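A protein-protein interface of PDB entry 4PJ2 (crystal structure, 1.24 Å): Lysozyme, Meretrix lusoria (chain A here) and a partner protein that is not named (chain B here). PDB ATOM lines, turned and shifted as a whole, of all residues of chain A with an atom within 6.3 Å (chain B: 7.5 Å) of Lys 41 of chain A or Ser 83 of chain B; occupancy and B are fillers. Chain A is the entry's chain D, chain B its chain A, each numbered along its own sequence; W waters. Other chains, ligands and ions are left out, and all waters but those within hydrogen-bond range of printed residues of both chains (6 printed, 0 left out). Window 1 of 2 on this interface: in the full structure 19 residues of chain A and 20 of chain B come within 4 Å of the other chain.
Water W1 lies within hydrogen-bond range of O of Gly 95 of chain A, OD2 of Asp 58 of chain B and OG of Ser 83 of chain B. Water W4 lies within hydrogen-bond range of the backbone carbonyl oxygen (O) of Ser 86 of chain B (2.7 Å) and the side-chain hydroxyl (OG) of Ser 34 of chain A (2.9 Å). Water W6 lies within hydrogen-bond range of the side-chain carboxylate of Asp 58 of chain B (2.7 Å) and the backbone carbonyl oxygen of Gly 95 of chain A (2.8 Å). Water W2 lies within hydrogen-bond range of the backbone carbonyl oxygen (O) of Ala 84 of chain B (2.8 Å), the backbone NH (N) of Lys 41 of chain A (2.9 Å) and the backbone carbonyl oxygen (O) of Gln 39 of chain A (3.5 Å). Water W5 lies within hydrogen-bond range of ND2 of Asn 94 of chain A and OH of Tyr 89 of chain B. Water W3 bridges the backbone carbonyl oxygen of Gln 39 of chain A (3.1 Å) and the backbone NH of Ser 86 of chain B (3.2 Å).
Leu 33 of chain A touches none of the printed residues of chain B. Of the printed residues of chain B, Gln 39 of chain A touches Ser 86 (3.9 Å). Ile 40 of chain A touches none of the printed residues of chain B. Printed residues of chain B within 4 Å of Lys 41 of chain A: Glu 82 (3.8 Å), Ser 83 (2.5 Å), Ala 84 (3.6 Å), Gly 85 (3.1 Å) and Ser 88 (2.6 Å). Of the printed residues of chain B, Tyr 44 of chain A touches Ala 84. Of the printed residues of chain B, Gly 95 of chain A touches Ser 83. Printed residues of chain A within 4 Å of Ser 83 of chain B: Lys 41, Gly 95 and Gly 96. Printed residues of chain A within 4 Å of Gly 85 of chain B: Lys 41, Asn 94 and Gly 96. Of the printed residues of chain A, Pro 114 of chain B touches Met 30. The nearest residue of chain A that does not touch Ser 83 of chain B is Asn 94 of chain A (4.6 Å).
O of Ala 27 of chain B is in hydrogen-bond range of OG of Ser 60 of chain B, at 3.1 Å. The backbone NH of Gly 59 of chain B sits at hydrogen-bond distance from the backbone carbonyl oxygen of Ser 28 of chain B. The backbone NH (N) of Glu 82 of chain B lies within hydrogen-bond range of the backbone carbonyl oxygen (O) of Ser 60 of chain B (2.9 Å). The backbone carbonyl oxygen of Tyr 89 of chain B lies within hydrogen-bond range of the backbone NH of Ser 83 of chain B (2.8 Å). The backbone carbonyl oxygen (O) of Leu 112 of chain B lies within hydrogen-bond range of the backbone NH (N) of Leu 90 of chain B, 2.9 Å away. The side-chain hydroxyl (OG) of Ser 34 of chain A lies within hydrogen-bond range of the backbone carbonyl oxygen (O) of Gln 39 of chain A (2.7 Å).
Among the printed residues, pairs that only touch across the chains: Met 30 of chain A with Glu 82 of chain B (3.2 Å), Met 30 of chain A with Ser 88 of chain B (3.6 Å), Met 30 of chain A with Leu 90 of chain B (3.7 Å), Gln 39 of chain A with Ser 86 of chain B (3.9 Å), Lys 41 of chain A with Glu 82 of chain B (3.8 Å), Lys 41 of chain A with Ala 84 of chain B (3.6 Å), Ala 43 of chain A with Ala 27 of chain B (3.7 Å), Ala 43 of chain A with Ser 28 of chain B (3.9 Å), Ala 43 of chain A with Ser 60 of chain B (3.9 Å), Tyr 44 of chain A with Ala 84 of chain B (3.7 Å), Asn 94 of chain A with Gly 85 of chain B (3.3 Å), Gly 96 of chain A with Ser 83 of chain B (3.9 Å), Gly 96 of chain A with Gly 85 of chain B (3.6 Å) and Pro 97 of chain A with Ser 28 of chain B (3.6 Å).
Of the 18 printed residues of chain A, 10 touch a printed residue of chain B. Hydrophobic or aromatic side chains of chain A that line the printed part of chain B: Met 30, Ala 43, Tyr 44 and Pro 97. Of the 19 printed residues of chain B, 14 touch a printed residue of chain A. Hydrophobic or aromatic side chains of chain B that line the printed part of chain A: Ala 27, Tyr 89, Leu 90 and Pro 114. Among the printed residues, no Asp or Glu carboxylate lies within 4 Å of a Lys or Arg side-chain nitrogen of the other chain.
The side-chain amino group (NZ) of Lys 62 of chain B lies within hydrogen-bond range of the side-chain sulfur (SD) of Met 30 of chain A, 3.2 Å away. The side-chain carboxylate (OE1) of Glu 82 of chain B is in hydrogen-bond range of the side-chain hydroxyl (OG) of Ser 32 of chain A, at 3.1 Å. NZ of Lys 41 of chain A lies within hydrogen-bond range of O of Ser 83 of chain B. OG of Ser 83 of chain B is in hydrogen-bond range of O of Gly 95 of chain A (3.1 Å). The side-chain amino group (NZ) of Lys 41 of chain A sits at hydrogen-bond distance from the backbone carbonyl oxygen (O) of Gly 85 of chain B, at 3.1 Å. The side-chain hydroxyl of Ser 86 of chain B lies within hydrogen-bond range of the side-chain amide nitrogen of Asn 94 of chain A, 3.0 Å away. The backbone carbonyl oxygen (O) of Asn 94 of chain A lies within hydrogen-bond range of the backbone NH (N) of Gly 87 of chain B (2.9 Å). OG of Ser 88 of chain B sits at hydrogen-bond distance from NZ of Lys 41 of chain A (2.6 Å). The side-chain hydroxyl (OH) of Tyr 89 of chain B lies within hydrogen-bond range of the side-chain amide oxygen (OD1) of Asn 94 of chain A, 2.7 Å away. The backbone carbonyl oxygen (O) of Pro 114 of chain B lies close to the side-chain sulfur (SD) of Met 30 of chain A, 2.6 Å away.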
ATOM      1  N   MET A  30      11.689   2.872  14.217  1.00  0.00           N
ATOM      2  CA  MET A  30      10.327   3.230  14.620  1.00  0.00           C
ATOM      3  C   MET A  30       9.686   2.235  15.579  1.00  0.00           C
ATOM      4  O   MET A  30       8.487   1.968  15.488  1.00  0.00           O
ATOM      5  CB  MET A  30       9.407   3.316  13.416  1.00  0.00           C
ATOM      6  CG  MET A  30       9.838   4.227  12.323  1.00  0.00           C
ATOM      7  SD  MET A  30       8.410   4.345  11.249  1.00  0.00           S
ATOM      8  CE  MET A  30       8.407   2.736  10.450  1.00  0.00           C
ATOM      9  N   SER A  32       9.883  -0.800  15.666  1.00  0.00           N
ATOM     10  CA  SER A  32       9.579  -2.045  14.975  1.00  0.00           C
ATOM     11  C   SER A  32      10.875  -2.759  14.610  1.00  0.00           C
ATOM     12  O   SER A  32      11.813  -2.138  14.109  1.00  0.00           O
ATOM     13  CB  SER A  32       8.771  -1.745  13.710  1.00  0.00           C
ATOM     14  OG  SER A  32       8.279  -2.933  13.129  1.00  0.00           O
ATOM     15  N   LEU A  33      10.928  -4.059  14.873  1.00  0.00           N
ATOM     16  CA  LEU A  33      12.115  -4.844  14.571  1.00  0.00           C
ATOM     17  C   LEU A  33      12.041  -5.501  13.196  1.00  0.00           C
ATOM     18  O   LEU A  33      11.006  -6.029  12.804  1.00  0.00           O
ATOM     19  CB  LEU A  33      12.303  -5.948  15.613  1.00  0.00           C
ATOM     20  CG  LEU A  33      12.897  -5.586  16.969  1.00  0.00           C
ATOM     21  CD1 LEU A  33      12.878  -6.801  17.884  1.00  0.00           C
ATOM     22  CD2 LEU A  33      14.313  -5.074  16.805  1.00  0.00           C
ATOM     23  N   SER A  34      13.157  -5.450  12.474  1.00  0.00           N
ATOM     24  CA  SER A  34      13.319  -6.190  11.233  1.00  0.00           C
ATOM     25  C   SER A  34      14.576  -7.026  11.392  1.00  0.00           C
ATOM     26  O   SER A  34      15.600  -6.523  11.873  1.00  0.00           O
ATOM     27  CB  SER A  34      13.457  -5.224  10.063  1.00  0.00           C
ATOM     28  OG  SER A  34      13.448  -5.908   8.830  1.00  0.00           O
ATOM     29  N   CYS A  35      14.508  -8.291  10.997  1.00  0.00           N
ATOM     30  CA  CYS A  35      15.549  -9.242  11.348  1.00  0.00           C
ATOM     31  C   CYS A  35      16.192  -9.969  10.173  1.00  0.00           C
ATOM     32  O   CYS A  35      15.523 -10.366   9.215  1.00  0.00           O
ATOM     33  CB  CYS A  35      14.975 -10.285  12.319  1.00  0.00           C
ATOM     34  SG  CYS A  35      14.194  -9.607  13.809  1.00  0.00           S
ATOM     35  N   GLN A  39      15.749  -9.149   6.222  1.00  0.00           N
ATOM     36  CA  GLN A  39      15.128  -8.040   6.960  1.00  0.00           C
ATOM     37  C   GLN A  39      13.598  -8.209   7.018  1.00  0.00           C
ATOM     38  O   GLN A  39      12.827  -7.351   6.579  1.00  0.00           O
ATOM     39  CB  GLN A  39      15.528  -6.711   6.330  1.00  0.00           C
ATOM     40  CG  GLN A  39      16.995  -6.372   6.574  1.00  0.00           C
ATOM     41  CD  GLN A  39      17.258  -6.070   8.033  1.00  0.00           C
ATOM     42  OE1 GLN A  39      16.910  -4.994   8.522  1.00  0.00           O
ATOM     43  NE2 GLN A  39      17.832  -7.028   8.745  1.00  0.00           N
ATOM     44  N   ILE A  40      13.203  -9.328   7.607  1.00  0.00           N
ATOM     45  CA  ILE A  40      11.803  -9.729   7.739  1.00  0.00           C
ATOM     46  C   ILE A  40      11.250  -9.224   9.062  1.00  0.00           C
ATOM     47  O   ILE A  40      11.897  -9.367  10.107  1.00  0.00           O
ATOM     48  CB  ILE A  40      11.703 -11.278   7.681  1.00  0.00           C
ATOM     49  CG1 ILE A  40      11.945 -11.750   6.249  1.00  0.00           C
ATOM     50  CG2 ILE A  40      10.346 -11.777   8.185  1.00  0.00           C
ATOM     51  CD1 ILE A  40      12.149 -13.251   6.123  1.00  0.00           C
ATOM     52  N   LYS A  41      10.063  -8.622   9.014  1.00  0.00           N
ATOM     53  CA  LYS A  41       9.376  -8.191  10.223  1.00  0.00           C
ATOM     54  C   LYS A  41       8.330  -9.222  10.630  1.00  0.00           C
ATOM     55  O   LYS A  41       8.016 -10.146   9.879  1.00  0.00           O
ATOM     56  CB  LYS A  41       8.731  -6.820  10.012  1.00  0.00           C
ATOM     57  CG  LYS A  41       9.758  -5.742   9.726  1.00  0.00           C
ATOM     58  CD  LYS A  41       9.165  -4.357   9.594  1.00  0.00           C
ATOM     59  CE  LYS A  41       8.248  -4.300   8.381  1.00  0.00           C
ATOM     60  NZ  LYS A  41       7.865  -2.924   8.007  1.00  0.00           N
ATOM     61  N   GLU A  42       7.798  -9.069  11.830  1.00  0.00           N
ATOM     62  CA  GLU A  42       6.897 -10.054  12.400  1.00  0.00           C
ATOM     63  C   GLU A  42       5.656 -10.276  11.528  1.00  0.00           C
ATOM     64  O   GLU A  42       5.231 -11.406  11.322  1.00  0.00           O
ATOM     65  CB  GLU A  42       6.488  -9.641  13.815  1.00  0.00           C
ATOM     66  CG  GLU A  42       5.785 -10.756  14.568  1.00  0.00           C
ATOM     67  CD  GLU A  42       5.524 -10.413  16.016  1.00  0.00           C
ATOM     68  OE1 GLU A  42       5.688  -9.233  16.389  1.00  0.00           O
ATOM     69  OE2 GLU A  42       5.157 -11.330  16.780  1.00  0.00           O
ATOM     70  N   ALA A  43       5.072  -9.194  11.019  1.00  0.00           N
ATOM     71  CA  ALA A  43       3.871  -9.298  10.195  1.00  0.00           C
ATOM     72  C   ALA A  43       4.127 -10.141   8.955  1.00  0.00           C
ATOM     73  O   ALA A  43       3.255 -10.887   8.489  1.00  0.00           O
ATOM     74  CB  ALA A  43       3.382  -7.926   9.795  1.00  0.00           C
ATOM     75  N   TYR A  44       5.322  -9.983   8.394  1.00  0.00           N
ATOM     76  CA  TYR A  44       5.728 -10.705   7.199  1.00  0.00           C
ATOM     77  C   TYR A  44       5.828 -12.190   7.521  1.00  0.00           C
ATOM     78  O   TYR A  44       5.289 -13.024   6.801  1.00  0.00           O
ATOM     79  CB  TYR A  44       7.047 -10.139   6.699  1.00  0.00           C
ATOM     80  CG  TYR A  44       7.539 -10.584   5.336  1.00  0.00           C
ATOM     81  CD1 TYR A  44       8.031 -11.864   5.134  1.00  0.00           C
ATOM     82  CD2 TYR A  44       7.622  -9.687   4.286  1.00  0.00           C
ATOM     83  CE1 TYR A  44       8.528 -12.252   3.902  1.00  0.00           C
ATOM     84  CE2 TYR A  44       8.126 -10.063   3.046  1.00  0.00           C
ATOM     85  CZ  TYR A  44       8.564 -11.349   2.862  1.00  0.00           C
ATOM     86  OH  TYR A  44       9.099 -11.728   1.656  1.00  0.00           O
ATOM     87  N   TRP A  45       6.480 -12.510   8.635  1.00  0.00           N
ATOM     88  CA  TRP A  45       6.641 -13.891   9.067  1.00  0.00           C
ATOM     89  C   TRP A  45       5.309 -14.568   9.343  1.00  0.00           C
ATOM     90  O   TRP A  45       5.106 -15.726   8.977  1.00  0.00           O
ATOM     91  CB  TRP A  45       7.535 -13.969  10.309  1.00  0.00           C
ATOM     92  CG  TRP A  45       7.774 -15.368  10.765  1.00  0.00           C
ATOM     93  CD1 TRP A  45       8.596 -16.285  10.186  1.00  0.00           C
ATOM     94  CD2 TRP A  45       7.174 -16.019  11.888  1.00  0.00           C
ATOM     95  NE1 TRP A  45       8.553 -17.467  10.885  1.00  0.00           N
ATOM     96  CE2 TRP A  45       7.687 -17.329  11.935  1.00  0.00           C
ATOM     97  CE3 TRP A  45       6.260 -15.618  12.866  1.00  0.00           C
ATOM     98  CZ2 TRP A  45       7.312 -18.243  12.920  1.00  0.00           C
ATOM     99  CZ3 TRP A  45       5.890 -16.525  13.840  1.00  0.00           C
ATOM    100  CH2 TRP A  45       6.419 -17.820  13.865  1.00  0.00           C
ATOM    101  N   ILE A  46       4.391 -13.843   9.966  1.00  0.00           N
ATOM    102  CA  ILE A  46       3.063 -14.378  10.235  1.00  0.00           C
ATOM    103  C   ILE A  46       2.379 -14.752   8.915  1.00  0.00           C
ATOM    104  O   ILE A  46       1.854 -15.855   8.763  1.00  0.00           O
ATOM    105  CB  ILE A  46       2.196 -13.368  11.038  1.00  0.00           C
ATOM    106  CG1 ILE A  46       2.722 -13.264  12.474  1.00  0.00           C
ATOM    107  CG2 ILE A  46       0.716 -13.758  11.012  1.00  0.00           C
ATOM    108  CD1 ILE A  46       2.133 -12.114  13.283  1.00  0.00           C
ATOM    109  N   TRP A  55       9.543 -16.144  14.661  1.00  0.00           N
ATOM    110  CA  TRP A  55       9.933 -15.115  13.711  1.00  0.00           C
ATOM    111  C   TRP A  55      11.450 -14.857  13.730  1.00  0.00           C
ATOM    112  O   TRP A  55      12.120 -14.944  12.701  1.00  0.00           O
ATOM    113  CB  TRP A  55       9.130 -13.858  14.030  1.00  0.00           C
ATOM    114  CG  TRP A  55       9.719 -12.573  13.609  1.00  0.00           C
ATOM    115  CD1 TRP A  55      10.343 -12.280  12.430  1.00  0.00           C
ATOM    116  CD2 TRP A  55       9.730 -11.380  14.379  1.00  0.00           C
ATOM    117  NE1 TRP A  55      10.742 -10.965  12.425  1.00  0.00           N
ATOM    118  CE2 TRP A  55      10.376 -10.392  13.615  1.00  0.00           C
ATOM    119  CE3 TRP A  55       9.246 -11.046  15.645  1.00  0.00           C
ATOM    120  CZ2 TRP A  55      10.554  -9.092  14.079  1.00  0.00           C
ATOM    121  CZ3 TRP A  55       9.429  -9.763  16.104  1.00  0.00           C
ATOM    122  CH2 TRP A  55      10.075  -8.798  15.322  1.00  0.00           C
ATOM    123  N   ASN A  94      10.070  -5.461  -0.570  1.00  0.00           N
ATOM    124  CA  ASN A  94      10.338  -4.140  -0.013  1.00  0.00           C
ATOM    125  C   ASN A  94       9.064  -3.406   0.394  1.00  0.00           C
ATOM    126  O   ASN A  94       9.074  -2.649   1.353  1.00  0.00           O
ATOM    127  CB  ASN A  94      11.102  -3.317  -1.057  1.00  0.00           C
ATOM    128  CG  ASN A  94      11.509  -1.948  -0.543  1.00  0.00           C
ATOM    129  OD1 ASN A  94      11.192  -0.933  -1.151  1.00  0.00           O
ATOM    130  ND2 ASN A  94      12.188  -1.923   0.582  1.00  0.00           N
ATOM    131  N   GLY A  95       7.978  -3.654  -0.345  1.00  0.00           N
ATOM    132  CA  GLY A  95       6.772  -2.853  -0.208  1.00  0.00           C
ATOM    133  C   GLY A  95       5.518  -3.533   0.293  1.00  0.00           C
ATOM    134  O   GLY A  95       4.502  -2.865   0.403  1.00  0.00           O
ATOM    135  N   GLY A  96       5.572  -4.829   0.594  1.00  0.00           N
ATOM    136  CA  GLY A  96       4.380  -5.551   1.043  1.00  0.00           C
ATOM    137  C   GLY A  96       3.560  -6.130  -0.094  1.00  0.00           C
ATOM    138  O   GLY A  96       4.018  -6.185  -1.227  1.00  0.00           O
ATOM    139  N   PRO A  97       2.326  -6.581   0.201  1.00  0.00           N
ATOM    140  CA  PRO A  97       1.539  -7.346  -0.772  1.00  0.00           C
ATOM    141  C   PRO A  97       1.262  -6.639  -2.081  1.00  0.00           C
ATOM    142  O   PRO A  97       1.043  -7.338  -3.064  1.00  0.00           O
ATOM    143  CB  PRO A  97       0.242  -7.610  -0.015  1.00  0.00           C
ATOM    144  CG  PRO A  97       0.688  -7.705   1.387  1.00  0.00           C
ATOM    145  CD  PRO A  97       1.678  -6.574   1.522  1.00  0.00           C
ATOM    146  N   ALA B  27      -1.844 -10.083   8.412  1.00  0.00           N
ATOM    147  CA  ALA B  27      -1.118  -9.026   9.078  1.00  0.00           C
ATOM    148  C   ALA B  27      -0.708  -7.896   8.137  1.00  0.00           C
ATOM    149  O   ALA B  27      -0.698  -6.743   8.535  1.00  0.00           O
ATOM    150  CB  ALA B  27       0.094  -9.595   9.784  1.00  0.00           C
ATOM    151  N   SER B  28      -0.370  -8.233   6.895  1.00  0.00           N
ATOM    152  CA  SER B  28       0.287  -7.281   6.000  1.00  0.00           C
ATOM    153  C   SER B  28      -0.653  -6.375   5.259  1.00  0.00           C
ATOM    154  O   SER B  28      -0.209  -5.384   4.677  1.00  0.00           O
ATOM    155  CB  SER B  28       1.105  -7.997   4.921  1.00  0.00           C
ATOM    156  OG  SER B  28       2.114  -8.829   5.436  1.00  0.00           O
ATOM    157  N   ASP B  58      -2.513  -0.664   4.179  1.00  0.00           N
ATOM    158  CA  ASP B  58      -1.338  -1.233   3.557  1.00  0.00           C
ATOM    159  C   ASP B  58      -0.291  -1.456   4.624  1.00  0.00           C
ATOM    160  O   ASP B  58       0.701  -0.700   4.745  1.00  0.00           O
ATOM    161  CB  ASP B  58      -0.811  -0.339   2.462  1.00  0.00           C
ATOM    162  CG  ASP B  58       0.391  -0.927   1.804  1.00  0.00           C
ATOM    163  OD1 ASP B  58       0.582  -2.163   1.905  1.00  0.00           O
ATOM    164  OD2 ASP B  58       1.149  -0.163   1.194  1.00  0.00           O
ATOM    165  N   GLY B  59      -0.525  -2.477   5.421  1.00  0.00           N
ATOM    166  CA  GLY B  59       0.354  -2.864   6.493  1.00  0.00           C
ATOM    167  C   GLY B  59      -0.437  -2.993   7.758  1.00  0.00           C
ATOM    168  O   GLY B  59      -1.641  -3.241   7.725  1.00  0.00           O
ATOM    169  N   SER B  60       0.245  -2.827   8.873  1.00  0.00           N
ATOM    170  CA  SER B  60      -0.338  -2.926  10.205  1.00  0.00           C
ATOM    171  C   SER B  60      -0.477  -1.543  10.837  1.00  0.00           C
ATOM    172  O   SER B  60       0.378  -0.671  10.640  1.00  0.00           O
ATOM    173  CB  SER B  60       0.578  -3.760  11.098  1.00  0.00           C
ATOM    174  OG  SER B  60       1.014  -4.927  10.442  1.00  0.00           O
ATOM    175  N   LYS B  62       0.163   1.146  13.270  1.00  0.00           N
ATOM    176  CA  LYS B  62       1.329   1.384  14.095  1.00  0.00           C
ATOM    177  C   LYS B  62       0.978   2.256  15.291  1.00  0.00           C
ATOM    178  O   LYS B  62       1.454   2.013  16.392  1.00  0.00           O
ATOM    179  CB  LYS B  62       2.399   2.063  13.247  1.00  0.00           C
ATOM    180  CG  LYS B  62       3.699   2.344  13.991  1.00  0.00           C
ATOM    181  CD  LYS B  62       4.597   3.330  13.241  1.00  0.00           C
ATOM    182  CE  LYS B  62       5.768   3.809  14.104  1.00  0.00           C
ATOM    183  NZ  LYS B  62       6.364   5.050  13.560  1.00  0.00           N
ATOM    184  N   VAL B  81      -0.157   3.690   9.523  1.00  0.00           N
ATOM    185  CA  VAL B  81      -0.007   2.297   9.120  1.00  0.00           C
ATOM    186  C   VAL B  81       1.393   2.078   8.561  1.00  0.00           C
ATOM    187  O   VAL B  81       1.872   2.889   7.778  1.00  0.00           O
ATOM    188  CB  VAL B  81      -1.056   1.930   8.047  1.00  0.00           C
ATOM    189  CG1 VAL B  81      -0.878   0.506   7.521  1.00  0.00           C
ATOM    190  CG2 VAL B  81      -2.456   2.079   8.632  1.00  0.00           C
ATOM    191  N   GLU B  82       2.017   0.973   8.959  1.00  0.00           N
ATOM    192  CA  GLU B  82       3.387   0.623   8.565  1.00  0.00           C
ATOM    193  C   GLU B  82       3.355  -0.568   7.604  1.00  0.00           C
ATOM    194  O   GLU B  82       2.831  -1.620   7.951  1.00  0.00           O
ATOM    195  CB  GLU B  82       4.190   0.264   9.829  1.00  0.00           C
ATOM    196  CG  GLU B  82       5.549  -0.419   9.613  1.00  0.00           C
ATOM    197  CD  GLU B  82       6.243  -0.779  10.923  1.00  0.00           C
ATOM    198  OE1 GLU B  82       5.931  -1.844  11.503  1.00  0.00           O
ATOM    199  OE2 GLU B  82       7.103   0.005  11.374  1.00  0.00           O
ATOM    200  N   SER B  83       3.959  -0.417   6.431  1.00  0.00           N
ATOM    201  CA  SER B  83       4.053  -1.501   5.455  1.00  0.00           C
ATOM    202  C   SER B  83       4.762  -2.698   6.041  1.00  0.00           C
ATOM    203  O   SER B  83       5.745  -2.542   6.794  1.00  0.00           O
ATOM    204  CB  SER B  83       4.824  -1.053   4.219  1.00  0.00           C
ATOM    205  OG  SER B  83       5.007  -2.173   3.370  1.00  0.00           O
ATOM    206  N   ALA B  84       4.309  -3.889   5.668  1.00  0.00           N
ATOM    207  CA  ALA B  84       4.918  -5.141   6.098  1.00  0.00           C
ATOM    208  C   ALA B  84       6.203  -5.457   5.351  1.00  0.00           C
ATOM    209  O   ALA B  84       6.912  -6.352   5.764  1.00  0.00           O
ATOM    210  CB  ALA B  84       3.944  -6.305   5.918  1.00  0.00           C
ATOM    211  N   GLY B  85       6.460  -4.763   4.240  1.00  0.00           N
ATOM    212  CA  GLY B  85       7.682  -4.967   3.478  1.00  0.00           C
ATOM    213  C   GLY B  85       8.889  -4.375   4.183  1.00  0.00           C
ATOM    214  O   GLY B  85       8.751  -3.626   5.155  1.00  0.00           O
ATOM    215  N   SER B  86      10.072  -4.731   3.696  1.00  0.00           N
ATOM    216  CA  SER B  86      11.324  -4.353   4.335  1.00  0.00           C
ATOM    217  C   SER B  86      11.480  -2.850   4.430  1.00  0.00           C
ATOM    218  O   SER B  86      12.205  -2.358   5.311  1.00  0.00           O
ATOM    219  CB  SER B  86      12.527  -4.952   3.563  1.00  0.00           C
ATOM    220  OG  SER B  86      12.677  -4.313   2.313  1.00  0.00           O
ATOM    221  N   GLY B  87      10.867  -2.113   3.515  1.00  0.00           N
ATOM    222  CA  GLY B  87      10.961  -0.667   3.474  1.00  0.00           C
ATOM    223  C   GLY B  87      10.210   0.037   4.587  1.00  0.00           C
ATOM    224  O   GLY B  87      10.476   1.208   4.871  1.00  0.00           O
ATOM    225  N   SER B  88       9.235  -0.643   5.191  1.00  0.00           N
ATOM    226  CA  SER B  88       8.536  -0.127   6.370  1.00  0.00           C
ATOM    227  C   SER B  88       7.856   1.203   6.095  1.00  0.00           C
ATOM    228  O   SER B  88       7.728   2.037   6.996  1.00  0.00           O
ATOM    229  CB  SER B  88       9.514  -0.017   7.544  1.00  0.00           C
ATOM    230  OG  SER B  88       9.946  -1.322   7.887  1.00  0.00           O
ATOM    231  N   TYR B  89       7.412   1.408   4.865  1.00  0.00           N
ATOM    232  CA  TYR B  89       6.845   2.684   4.464  1.00  0.00           C
ATOM    233  C   TYR B  89       5.582   2.999   5.249  1.00  0.00           C
ATOM    234  O   TYR B  89       4.758   2.122   5.549  1.00  0.00           O
ATOM    235  CB  TYR B  89       6.525   2.695   2.974  1.00  0.00           C
ATOM    236  CG  TYR B  89       7.741   2.358   2.146  1.00  0.00           C
ATOM    237  CD1 TYR B  89       8.805   3.250   2.050  1.00  0.00           C
ATOM    238  CD2 TYR B  89       7.850   1.151   1.469  1.00  0.00           C
ATOM    239  CE1 TYR B  89       9.942   2.955   1.320  1.00  0.00           C
ATOM    240  CE2 TYR B  89       8.991   0.853   0.723  1.00  0.00           C
ATOM    241  CZ  TYR B  89      10.031   1.772   0.662  1.00  0.00           C
ATOM    242  OH  TYR B  89      11.186   1.544  -0.042  1.00  0.00           O
ATOM    243  N   LEU B  90       5.432   4.272   5.577  1.00  0.00           N
ATOM    244  CA  LEU B  90       4.278   4.725   6.344  1.00  0.00           C
ATOM    245  C   LEU B  90       3.211   5.303   5.447  1.00  0.00           C
ATOM    246  O   LEU B  90       3.450   5.982   4.455  1.00  0.00           O
ATOM    247  CB  LEU B  90       4.703   5.784   7.372  1.00  0.00           C
ATOM    248  CG  LEU B  90       5.701   5.317   8.436  1.00  0.00           C
ATOM    249  CD1 LEU B  90       6.064   6.477   9.364  1.00  0.00           C
ATOM    250  CD2 LEU B  90       5.193   4.149   9.250  1.00  0.00           C
ATOM    251  N   SER B  91       1.976   5.028   5.849  1.00  0.00           N
ATOM    252  CA  SER B  91       0.811   5.659   5.265  1.00  0.00           C
ATOM    253  C   SER B  91      -0.056   6.115   6.422  1.00  0.00           C
ATOM    254  O   SER B  91       0.141   5.703   7.565  1.00  0.00           O
ATOM    255  CB  SER B  91       0.072   4.689   4.329  1.00  0.00           C
ATOM    256  OG  SER B  91      -0.263   3.481   4.995  1.00  0.00           O
ATOM    257  N   LEU B 112       5.696   6.975   2.627  1.00  0.00           N
ATOM    258  CA  LEU B 112       6.646   7.798   3.388  1.00  0.00           C
ATOM    259  C   LEU B 112       7.737   6.938   3.962  1.00  0.00           C
ATOM    260  O   LEU B 112       7.534   5.795   4.312  1.00  0.00           O
ATOM    261  CB  LEU B 112       5.922   8.454   4.560  1.00  0.00           C
ATOM    262  CG  LEU B 112       5.178   9.765   4.346  1.00  0.00           C
ATOM    263  CD1 LEU B 112       4.314   9.781   3.147  1.00  0.00           C
ATOM    264  CD2 LEU B 112       4.343  10.070   5.572  1.00  0.00           C
ATOM    265  N   PRO B 114      10.317   5.476   6.766  1.00  0.00           N
ATOM    266  CA  PRO B 114       9.996   5.107   8.158  1.00  0.00           C
ATOM    267  C   PRO B 114       9.997   6.266   9.168  1.00  0.00           C
ATOM    268  O   PRO B 114       9.100   6.502   9.963  1.00  0.00           O
ATOM    269  CB  PRO B 114      11.120   4.126   8.496  1.00  0.00           C
ATOM    270  CG  PRO B 114      11.415   3.458   7.207  1.00  0.00           C
ATOM    271  CD  PRO B 114      11.176   4.463   6.119  1.00  0.00           C
HETATM  272  O   HOH W   1       3.840  -0.416   0.947  1.00  0.00           O
HETATM  273  O   HOH W   2       9.369  -7.504   6.480  1.00  0.00           O
HETATM  274  O   HOH W   3      10.779  -7.749   4.310  1.00  0.00           O
HETATM  275  O   HOH W   4      12.893  -3.317   7.717  1.00  0.00           O
HETATM  276  O   HOH W   5      13.678   0.556   1.524  1.00  0.00           O
HETATM  277  O   HOH W   6       1.839  -3.315  -0.215  1.00  0.00           O
